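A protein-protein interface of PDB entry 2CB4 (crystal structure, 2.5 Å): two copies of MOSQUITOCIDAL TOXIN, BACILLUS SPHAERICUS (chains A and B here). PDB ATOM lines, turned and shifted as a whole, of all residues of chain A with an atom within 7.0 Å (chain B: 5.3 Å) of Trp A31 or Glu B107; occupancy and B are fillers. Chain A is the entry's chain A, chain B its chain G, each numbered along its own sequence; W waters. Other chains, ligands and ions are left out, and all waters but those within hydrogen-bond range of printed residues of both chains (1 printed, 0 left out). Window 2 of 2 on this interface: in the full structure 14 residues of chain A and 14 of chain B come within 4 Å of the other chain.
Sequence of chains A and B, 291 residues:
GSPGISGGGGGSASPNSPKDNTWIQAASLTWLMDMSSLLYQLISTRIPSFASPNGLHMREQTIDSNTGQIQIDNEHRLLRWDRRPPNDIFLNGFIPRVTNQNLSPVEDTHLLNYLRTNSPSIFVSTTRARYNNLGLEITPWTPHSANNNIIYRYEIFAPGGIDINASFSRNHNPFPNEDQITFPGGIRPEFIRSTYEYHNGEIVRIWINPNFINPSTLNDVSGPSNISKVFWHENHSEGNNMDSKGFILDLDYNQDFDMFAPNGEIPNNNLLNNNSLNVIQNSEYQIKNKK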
ATOM      1  N   ALA A  27      -3.747  24.434  24.045  1.00  0.00           N
ATOM      2  CA  ALA A  27      -3.003  23.340  23.442  1.00  0.00           C
ATOM      3  C   ALA A  27      -3.749  22.226  22.747  1.00  0.00           C
ATOM      4  O   ALA A  27      -4.678  21.597  23.299  1.00  0.00           O
ATOM      5  CB  ALA A  27      -1.963  22.758  24.399  1.00  0.00           C
ATOM      6  N   SER A  28      -3.259  21.959  21.550  1.00  0.00           N
ATOM      7  CA  SER A  28      -3.709  20.875  20.700  1.00  0.00           C
ATOM      8  C   SER A  28      -2.939  19.620  21.198  1.00  0.00           C
ATOM      9  O   SER A  28      -3.515  18.549  21.318  1.00  0.00           O
ATOM     10  CB  SER A  28      -3.328  21.168  19.249  1.00  0.00           C
ATOM     11  OG  SER A  28      -4.047  20.287  18.455  1.00  0.00           O
ATOM     12  N   LEU A  29      -1.643  19.779  21.516  1.00  0.00           N
ATOM     13  CA  LEU A  29      -0.823  18.692  22.093  1.00  0.00           C
ATOM     14  C   LEU A  29      -1.185  18.735  23.584  1.00  0.00           C
ATOM     15  O   LEU A  29      -0.492  19.353  24.387  1.00  0.00           O
ATOM     16  CB  LEU A  29       0.676  19.008  21.912  1.00  0.00           C
ATOM     17  CG  LEU A  29       1.161  19.241  20.470  1.00  0.00           C
ATOM     18  CD1 LEU A  29       2.692  19.337  20.407  1.00  0.00           C
ATOM     19  CD2 LEU A  29       0.633  18.115  19.562  1.00  0.00           C
ATOM     20  N   THR A  30      -2.330  18.154  23.918  1.00  0.00           N
ATOM     21  CA  THR A  30      -2.893  18.188  25.273  1.00  0.00           C
ATOM     22  C   THR A  30      -2.009  17.657  26.401  1.00  0.00           C
ATOM     23  O   THR A  30      -2.150  18.063  27.548  1.00  0.00           O
ATOM     24  CB  THR A  30      -4.268  17.507  25.318  1.00  0.00           C
ATOM     25  OG1 THR A  30      -4.131  16.159  24.853  1.00  0.00           O
ATOM     26  CG2 THR A  30      -5.268  18.255  24.428  1.00  0.00           C
ATOM     27  N   TRP A  31      -1.103  16.757  26.069  1.00  0.00           N
ATOM     28  CA  TRP A  31      -0.203  16.212  27.065  1.00  0.00           C
ATOM     29  C   TRP A  31       0.739  17.270  27.640  1.00  0.00           C
ATOM     30  O   TRP A  31       1.309  17.072  28.707  1.00  0.00           O
ATOM     31  CB  TRP A  31       0.578  15.026  26.501  1.00  0.00           C
ATOM     32  CG  TRP A  31       1.112  15.245  25.121  1.00  0.00           C
ATOM     33  CD1 TRP A  31       0.504  14.903  23.931  1.00  0.00           C
ATOM     34  CD2 TRP A  31       2.378  15.827  24.773  1.00  0.00           C
ATOM     35  NE1 TRP A  31       1.325  15.246  22.880  1.00  0.00           N
ATOM     36  CE2 TRP A  31       2.469  15.824  23.364  1.00  0.00           C
ATOM     37  CE3 TRP A  31       3.433  16.371  25.521  1.00  0.00           C
ATOM     38  CZ2 TRP A  31       3.569  16.314  22.690  1.00  0.00           C
ATOM     39  CZ3 TRP A  31       4.528  16.881  24.844  1.00  0.00           C
ATOM     40  CH2 TRP A  31       4.585  16.854  23.441  1.00  0.00           C
ATOM     41  N   LEU A  32       0.890  18.394  26.947  1.00  0.00           N
ATOM     42  CA  LEU A  32       1.754  19.475  27.425  1.00  0.00           C
ATOM     43  C   LEU A  32       1.112  20.201  28.599  1.00  0.00           C
ATOM     44  O   LEU A  32       1.807  20.748  29.445  1.00  0.00           O
ATOM     45  CB  LEU A  32       1.930  20.519  26.325  1.00  0.00           C
ATOM     46  CG  LEU A  32       3.011  20.318  25.278  1.00  0.00           C
ATOM     47  CD1 LEU A  32       3.096  21.598  24.483  1.00  0.00           C
ATOM     48  CD2 LEU A  32       4.343  19.996  25.957  1.00  0.00           C
ATOM     49  N   MET A  33      -0.215  20.276  28.602  1.00  0.00           N
ATOM     50  CA  MET A  33      -0.949  21.013  29.636  1.00  0.00           C
ATOM     51  C   MET A  33      -0.684  20.634  31.098  1.00  0.00           C
ATOM     52  O   MET A  33      -0.854  21.459  32.005  1.00  0.00           O
ATOM     53  CB  MET A  33      -2.441  21.139  29.331  1.00  0.00           C
ATOM     54  CG  MET A  33      -2.840  21.553  27.922  1.00  0.00           C
ATOM     55  SD  MET A  33      -4.724  21.868  27.854  1.00  0.00           S
ATOM     56  CE  MET A  33      -5.343  20.212  28.455  1.00  0.00           C
ATOM     57  N   ASP A  34      -0.285  19.391  31.331  1.00  0.00           N
ATOM     58  CA  ASP A  34      -0.008  18.934  32.694  1.00  0.00           C
ATOM     59  C   ASP A  34       1.484  19.026  33.047  1.00  0.00           C
ATOM     60  O   ASP A  34       1.902  18.625  34.141  1.00  0.00           O
ATOM     61  CB  ASP A  34      -0.471  17.491  32.862  1.00  0.00           C
ATOM     62  CG  ASP A  34      -1.925  17.393  33.315  1.00  0.00           C
ATOM     63  OD1 ASP A  34      -2.673  18.405  33.229  1.00  0.00           O
ATOM     64  OD2 ASP A  34      -2.294  16.299  33.793  1.00  0.00           O
ATOM     65  N   MET A  35       2.280  19.546  32.113  1.00  0.00           N
ATOM     66  CA  MET A  35       3.709  19.655  32.305  1.00  0.00           C
ATOM     67  C   MET A  35       4.129  21.105  32.147  1.00  0.00           C
ATOM     68  O   MET A  35       5.193  21.409  31.640  1.00  0.00           O
ATOM     69  CB  MET A  35       4.365  18.635  31.386  1.00  0.00           C
ATOM     70  CG  MET A  35       4.774  19.078  30.011  1.00  0.00           C
ATOM     71  SD  MET A  35       5.654  17.655  29.078  1.00  0.00           S
ATOM     72  CE  MET A  35       4.397  16.391  29.673  1.00  0.00           C
ATOM     73  N   SER A  36       3.265  22.000  32.615  1.00  0.00           N
ATOM     74  CA  SER A  36       3.479  23.427  32.540  1.00  0.00           C
ATOM     75  C   SER A  36       4.827  23.929  33.056  1.00  0.00           C
ATOM     76  O   SER A  36       5.553  24.642  32.359  1.00  0.00           O
ATOM     77  CB  SER A  36       2.330  24.176  33.231  1.00  0.00           C
ATOM     78  OG  SER A  36       2.632  25.565  33.356  1.00  0.00           O
ATOM     79  N   VAL A  98       5.828  19.979  15.029  1.00  0.00           N
ATOM     80  CA  VAL A  98       6.383  18.875  15.824  1.00  0.00           C
ATOM     81  C   VAL A  98       5.268  18.442  16.802  1.00  0.00           C
ATOM     82  O   VAL A  98       4.717  19.254  17.538  1.00  0.00           O
ATOM     83  CB  VAL A  98       7.654  19.299  16.591  1.00  0.00           C
ATOM     84  CG1 VAL A  98       8.093  18.207  17.566  1.00  0.00           C
ATOM     85  CG2 VAL A  98       8.773  19.634  15.622  1.00  0.00           C
ATOM     86  N   THR A  99       4.904  17.164  16.762  1.00  0.00           N
ATOM     87  CA  THR A  99       3.817  16.635  17.588  1.00  0.00           C
ATOM     88  C   THR A  99       4.213  15.526  18.588  1.00  0.00           C
ATOM     89  O   THR A  99       3.399  15.084  19.398  1.00  0.00           O
ATOM     90  CB  THR A  99       2.657  16.097  16.678  1.00  0.00           C
ATOM     91  OG1 THR A  99       3.148  15.026  15.863  1.00  0.00           O
ATOM     92  CG2 THR A  99       2.114  17.214  15.753  1.00  0.00           C
ATOM     93  N   ASN A 100       5.449  15.069  18.536  1.00  0.00           N
ATOM     94  CA  ASN A 100       5.882  13.993  19.433  1.00  0.00           C
ATOM     95  C   ASN A 100       6.522  14.492  20.727  1.00  0.00           C
ATOM     96  O   ASN A 100       7.157  15.548  20.742  1.00  0.00           O
ATOM     97  CB  ASN A 100       6.844  13.045  18.703  1.00  0.00           C
ATOM     98  CG  ASN A 100       8.187  13.703  18.395  1.00  0.00           C
ATOM     99  OD1 ASN A 100       8.263  14.629  17.584  1.00  0.00           O
ATOM    100  ND2 ASN A 100       9.240  13.256  19.077  1.00  0.00           N
ATOM    101  N   GLN A 101       6.365  13.734  21.811  1.00  0.00           N
ATOM    102  CA  GLN A 101       6.980  14.144  23.072  1.00  0.00           C
ATOM    103  C   GLN A 101       8.514  14.002  23.082  1.00  0.00           C
ATOM    104  O   GLN A 101       9.076  12.982  22.678  1.00  0.00           O
ATOM    105  CB  GLN A 101       6.353  13.483  24.299  1.00  0.00           C
ATOM    106  CG  GLN A 101       6.772  14.169  25.622  1.00  0.00           C
ATOM    107  CD  GLN A 101       6.082  13.593  26.853  1.00  0.00           C
ATOM    108  OE1 GLN A 101       6.585  12.662  27.470  1.00  0.00           O
ATOM    109  NE2 GLN A 101       4.960  14.188  27.240  1.00  0.00           N
ATOM    110  N   ASN A 102       9.180  15.061  23.515  1.00  0.00           N
ATOM    111  CA  ASN A 102      10.633  15.074  23.591  1.00  0.00           C
ATOM    112  C   ASN A 102      11.063  16.124  24.627  1.00  0.00           C
ATOM    113  O   ASN A 102      11.141  17.336  24.318  1.00  0.00           O
ATOM    114  CB  ASN A 102      11.249  15.332  22.216  1.00  0.00           C
ATOM    115  CG  ASN A 102      12.783  15.344  22.236  1.00  0.00           C
ATOM    116  OD1 ASN A 102      13.404  15.806  23.193  1.00  0.00           O
ATOM    117  ND2 ASN A 102      13.383  14.855  21.159  1.00  0.00           N
ATOM    118  N   LEU A 103      11.322  15.636  25.850  1.00  0.00           N
ATOM    119  CA  LEU A 103      11.724  16.466  27.002  1.00  0.00           C
ATOM    120  C   LEU A 103      13.217  16.840  27.016  1.00  0.00           C
ATOM    121  O   LEU A 103      13.781  17.200  28.058  1.00  0.00           O
ATOM    122  CB  LEU A 103      11.262  15.840  28.329  1.00  0.00           C
ATOM    123  CG  LEU A 103       9.754  15.542  28.410  1.00  0.00           C
ATOM    124  CD1 LEU A 103       9.396  14.721  29.646  1.00  0.00           C
ATOM    125  CD2 LEU A 103       8.903  16.802  28.316  1.00  0.00           C
ATOM    126  N   ILE A 122       7.126  22.942  18.490  1.00  0.00           N
ATOM    127  CA  ILE A 122       5.818  22.715  19.091  1.00  0.00           C
ATOM    128  C   ILE A 122       4.998  24.019  19.145  1.00  0.00           C
ATOM    129  O   ILE A 122       3.876  24.030  19.652  1.00  0.00           O
ATOM    130  CB  ILE A 122       5.961  22.183  20.544  1.00  0.00           C
ATOM    131  CG1 ILE A 122       6.714  23.187  21.436  1.00  0.00           C
ATOM    132  CG2 ILE A 122       6.619  20.804  20.574  1.00  0.00           C
ATOM    133  CD1 ILE A 122       6.367  23.053  22.950  1.00  0.00           C
ATOM    134  N   PRO B 105       0.391   6.940  33.201  1.00  0.00           N
ATOM    135  CA  PRO B 105      -0.448   8.135  33.376  1.00  0.00           C
ATOM    136  C   PRO B 105      -0.539   8.985  32.094  1.00  0.00           C
ATOM    137  O   PRO B 105      -0.771  10.207  32.152  1.00  0.00           O
ATOM    138  CB  PRO B 105       0.252   8.903  34.511  1.00  0.00           C
ATOM    139  CG  PRO B 105       1.719   8.493  34.411  1.00  0.00           C
ATOM    140  CD  PRO B 105       1.763   7.123  33.740  1.00  0.00           C
ATOM    141  N   VAL B 106      -0.387   8.320  30.944  1.00  0.00           N
ATOM    142  CA  VAL B 106      -0.479   8.971  29.640  1.00  0.00           C
ATOM    143  C   VAL B 106      -1.878   9.600  29.524  1.00  0.00           C
ATOM    144  O   VAL B 106      -2.704   9.518  30.450  1.00  0.00           O
ATOM    145  CB  VAL B 106      -0.276   7.937  28.488  1.00  0.00           C
ATOM    146  CG1 VAL B 106       1.160   7.482  28.441  1.00  0.00           C
ATOM    147  CG2 VAL B 106      -1.186   6.730  28.684  1.00  0.00           C
ATOM    148  N   GLU B 107      -2.147  10.214  28.377  1.00  0.00           N
ATOM    149  CA  GLU B 107      -3.441  10.833  28.137  1.00  0.00           C
ATOM    150  C   GLU B 107      -4.608   9.837  28.020  1.00  0.00           C
ATOM    151  O   GLU B 107      -5.766  10.229  28.154  1.00  0.00           O
ATOM    152  CB  GLU B 107      -3.389  11.714  26.881  1.00  0.00           C
ATOM    153  CG  GLU B 107      -2.507  12.955  27.017  1.00  0.00           C
ATOM    154  CD  GLU B 107      -2.937  13.871  28.148  1.00  0.00           C
ATOM    155  OE1 GLU B 107      -4.032  14.468  28.018  1.00  0.00           O
ATOM    156  OE2 GLU B 107      -2.179  13.999  29.147  1.00  0.00           O
ATOM    157  N   ASP B 108      -4.298   8.567  27.749  1.00  0.00           N
ATOM    158  CA  ASP B 108      -5.307   7.515  27.575  1.00  0.00           C
ATOM    159  C   ASP B 108      -6.392   7.502  28.631  1.00  0.00           C
ATOM    160  O   ASP B 108      -7.560   7.268  28.327  1.00  0.00           O
ATOM    161  CB  ASP B 108      -4.660   6.129  27.522  1.00  0.00           C
ATOM    162  CG  ASP B 108      -3.662   5.974  26.381  1.00  0.00           C
ATOM    163  OD1 ASP B 108      -3.429   6.958  25.637  1.00  0.00           O
ATOM    164  OD2 ASP B 108      -3.092   4.864  26.234  1.00  0.00           O
ATOM    165  N   THR B 109      -5.988   7.715  29.881  1.00  0.00           N
ATOM    166  CA  THR B 109      -6.909   7.687  31.026  1.00  0.00           C
ATOM    167  C   THR B 109      -7.162   9.046  31.618  1.00  0.00           C
ATOM    168  O   THR B 109      -7.837   9.162  32.619  1.00  0.00           O
ATOM    169  CB  THR B 109      -6.406   6.739  32.154  1.00  0.00           C
ATOM    170  OG1 THR B 109      -5.056   7.078  32.505  1.00  0.00           O
ATOM    171  CG2 THR B 109      -6.434   5.302  31.669  1.00  0.00           C
ATOM    172  N   HIS B 110      -6.632  10.082  30.982  1.00  0.00           N
ATOM    173  CA  HIS B 110      -6.821  11.430  31.467  1.00  0.00           C
ATOM    174  C   HIS B 110      -8.228  11.958  31.225  1.00  0.00           C
ATOM    175  O   HIS B 110      -8.516  12.634  30.235  1.00  0.00           O
ATOM    176  CB  HIS B 110      -5.743  12.375  30.936  1.00  0.00           C
ATOM    177  CG  HIS B 110      -5.640  13.641  31.716  1.00  0.00           C
ATOM    178  ND1 HIS B 110      -4.442  14.309  31.911  1.00  0.00           N
ATOM    179  CD2 HIS B 110      -6.584  14.361  32.384  1.00  0.00           C
ATOM    180  CE1 HIS B 110      -4.660  15.395  32.643  1.00  0.00           C
ATOM    181  NE2 HIS B 110      -5.949  15.444  32.949  1.00  0.00           N
ATOM    182  N   ASN B 113      -8.897  15.910  30.680  1.00  0.00           N
ATOM    183  CA  ASN B 113      -8.356  16.366  29.398  1.00  0.00           C
ATOM    184  C   ASN B 113      -9.310  15.855  28.288  1.00  0.00           C
ATOM    185  O   ASN B 113      -9.601  16.572  27.315  1.00  0.00           O
ATOM    186  CB  ASN B 113      -6.913  15.835  29.231  1.00  0.00           C
ATOM    187  CG  ASN B 113      -5.825  16.909  29.568  1.00  0.00           C
ATOM    188  OD1 ASN B 113      -6.083  17.931  30.230  1.00  0.00           O
ATOM    189  ND2 ASN B 113      -4.621  16.699  29.053  1.00  0.00           N
ATOM    190  N   SER B 119      -9.334  14.767  23.425  1.00  0.00           N
ATOM    191  CA  SER B 119      -8.122  14.032  23.075  1.00  0.00           C
ATOM    192  C   SER B 119      -8.466  12.521  23.072  1.00  0.00           C
ATOM    193  O   SER B 119      -9.379  12.092  23.763  1.00  0.00           O
ATOM    194  CB  SER B 119      -7.056  14.336  24.151  1.00  0.00           C
ATOM    195  OG  SER B 119      -7.614  14.248  25.471  1.00  0.00           O
ATOM    196  N   PRO B 120      -7.745  11.723  22.295  1.00  0.00           N
ATOM    197  CA  PRO B 120      -8.007  10.270  22.216  1.00  0.00           C
ATOM    198  C   PRO B 120      -7.831   9.603  23.565  1.00  0.00           C
ATOM    199  O   PRO B 120      -6.847   9.853  24.278  1.00  0.00           O
ATOM    200  CB  PRO B 120      -6.931   9.753  21.248  1.00  0.00           C
ATOM    201  CG  PRO B 120      -6.442  10.964  20.539  1.00  0.00           C
ATOM    202  CD  PRO B 120      -6.637  12.145  21.419  1.00  0.00           C
ATOM    203  N   SER B 121      -8.768   8.723  23.908  1.00  0.00           N
ATOM    204  CA  SER B 121      -8.695   8.058  25.190  1.00  0.00           C
ATOM    205  C   SER B 121      -9.462   6.760  25.144  1.00  0.00           C
ATOM    206  O   SER B 121      -9.985   6.375  24.101  1.00  0.00           O
ATOM    207  CB  SER B 121      -9.303   8.976  26.253  1.00  0.00           C
ATOM    208  OG  SER B 121     -10.702   9.074  26.095  1.00  0.00           O
HETATM  209  O   HOH W   1      -4.868  19.748  32.292  1.00  0.00           O
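The side-chain amide nitrogen of Asn B113 lies within hydrogen-bond range of the backbone carbonyl oxygen of Thr A30 (3.2 Å).
OD2 of Asp A34 sits close to ND1 of His B110.
ND2 of Asn B113 is in hydrogen-bond range of OE1 of Glu B107.
Among the printed residues, merely in contact across the chains: Thr A30 with Glu B107, Thr A30 with Ser B119, Trp A31 with Glu B107 and Met A33 with Asn B113.
Of chain B, only Glu B107 comes within 4 Å of Trp A31.
Of the printed residues of chain B, Asp A34 touches His B110.
Asn A100 touches none of the printed residues of chain B.
Of chain A, only Thr A30 (3.6 Å) and Trp A31 (3.6 Å) come within 4 Å of Glu B107.
Of the printed residues of chain A, Ser B119 touches Thr A30 (3.5 Å).
The nearest printed residue of chain B that does not touch Met A33 is Glu B107 (5.9 Å).
Of the 17 printed residues of chain A, 4 touch a printed residue of chain B.
Hydrophobic or aromatic side chains of chain A that line the printed part of chain B: Trp A31 and Met A33.
Of the 10 printed residues of chain B, 4 touch a printed residue of chain A.
Printed residues of chain B that touch a printed residue of chain A: Glu B107, His B110, Asn B113 and Ser B119.
Hydrophobic or aromatic side chains of chain B that line the printed part of chain A: His B110.
No position is printed for both chains.
Of the 6 pairs that touch across the chains among the printed residues, none has its exchanged pair printed and touching as well.
Water W1 bridges the side-chain carboxylate (OD1) of Asp A34 (2.7 Å) and the side-chain amide oxygen (OD1) of Asn B113 (3.0 Å).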
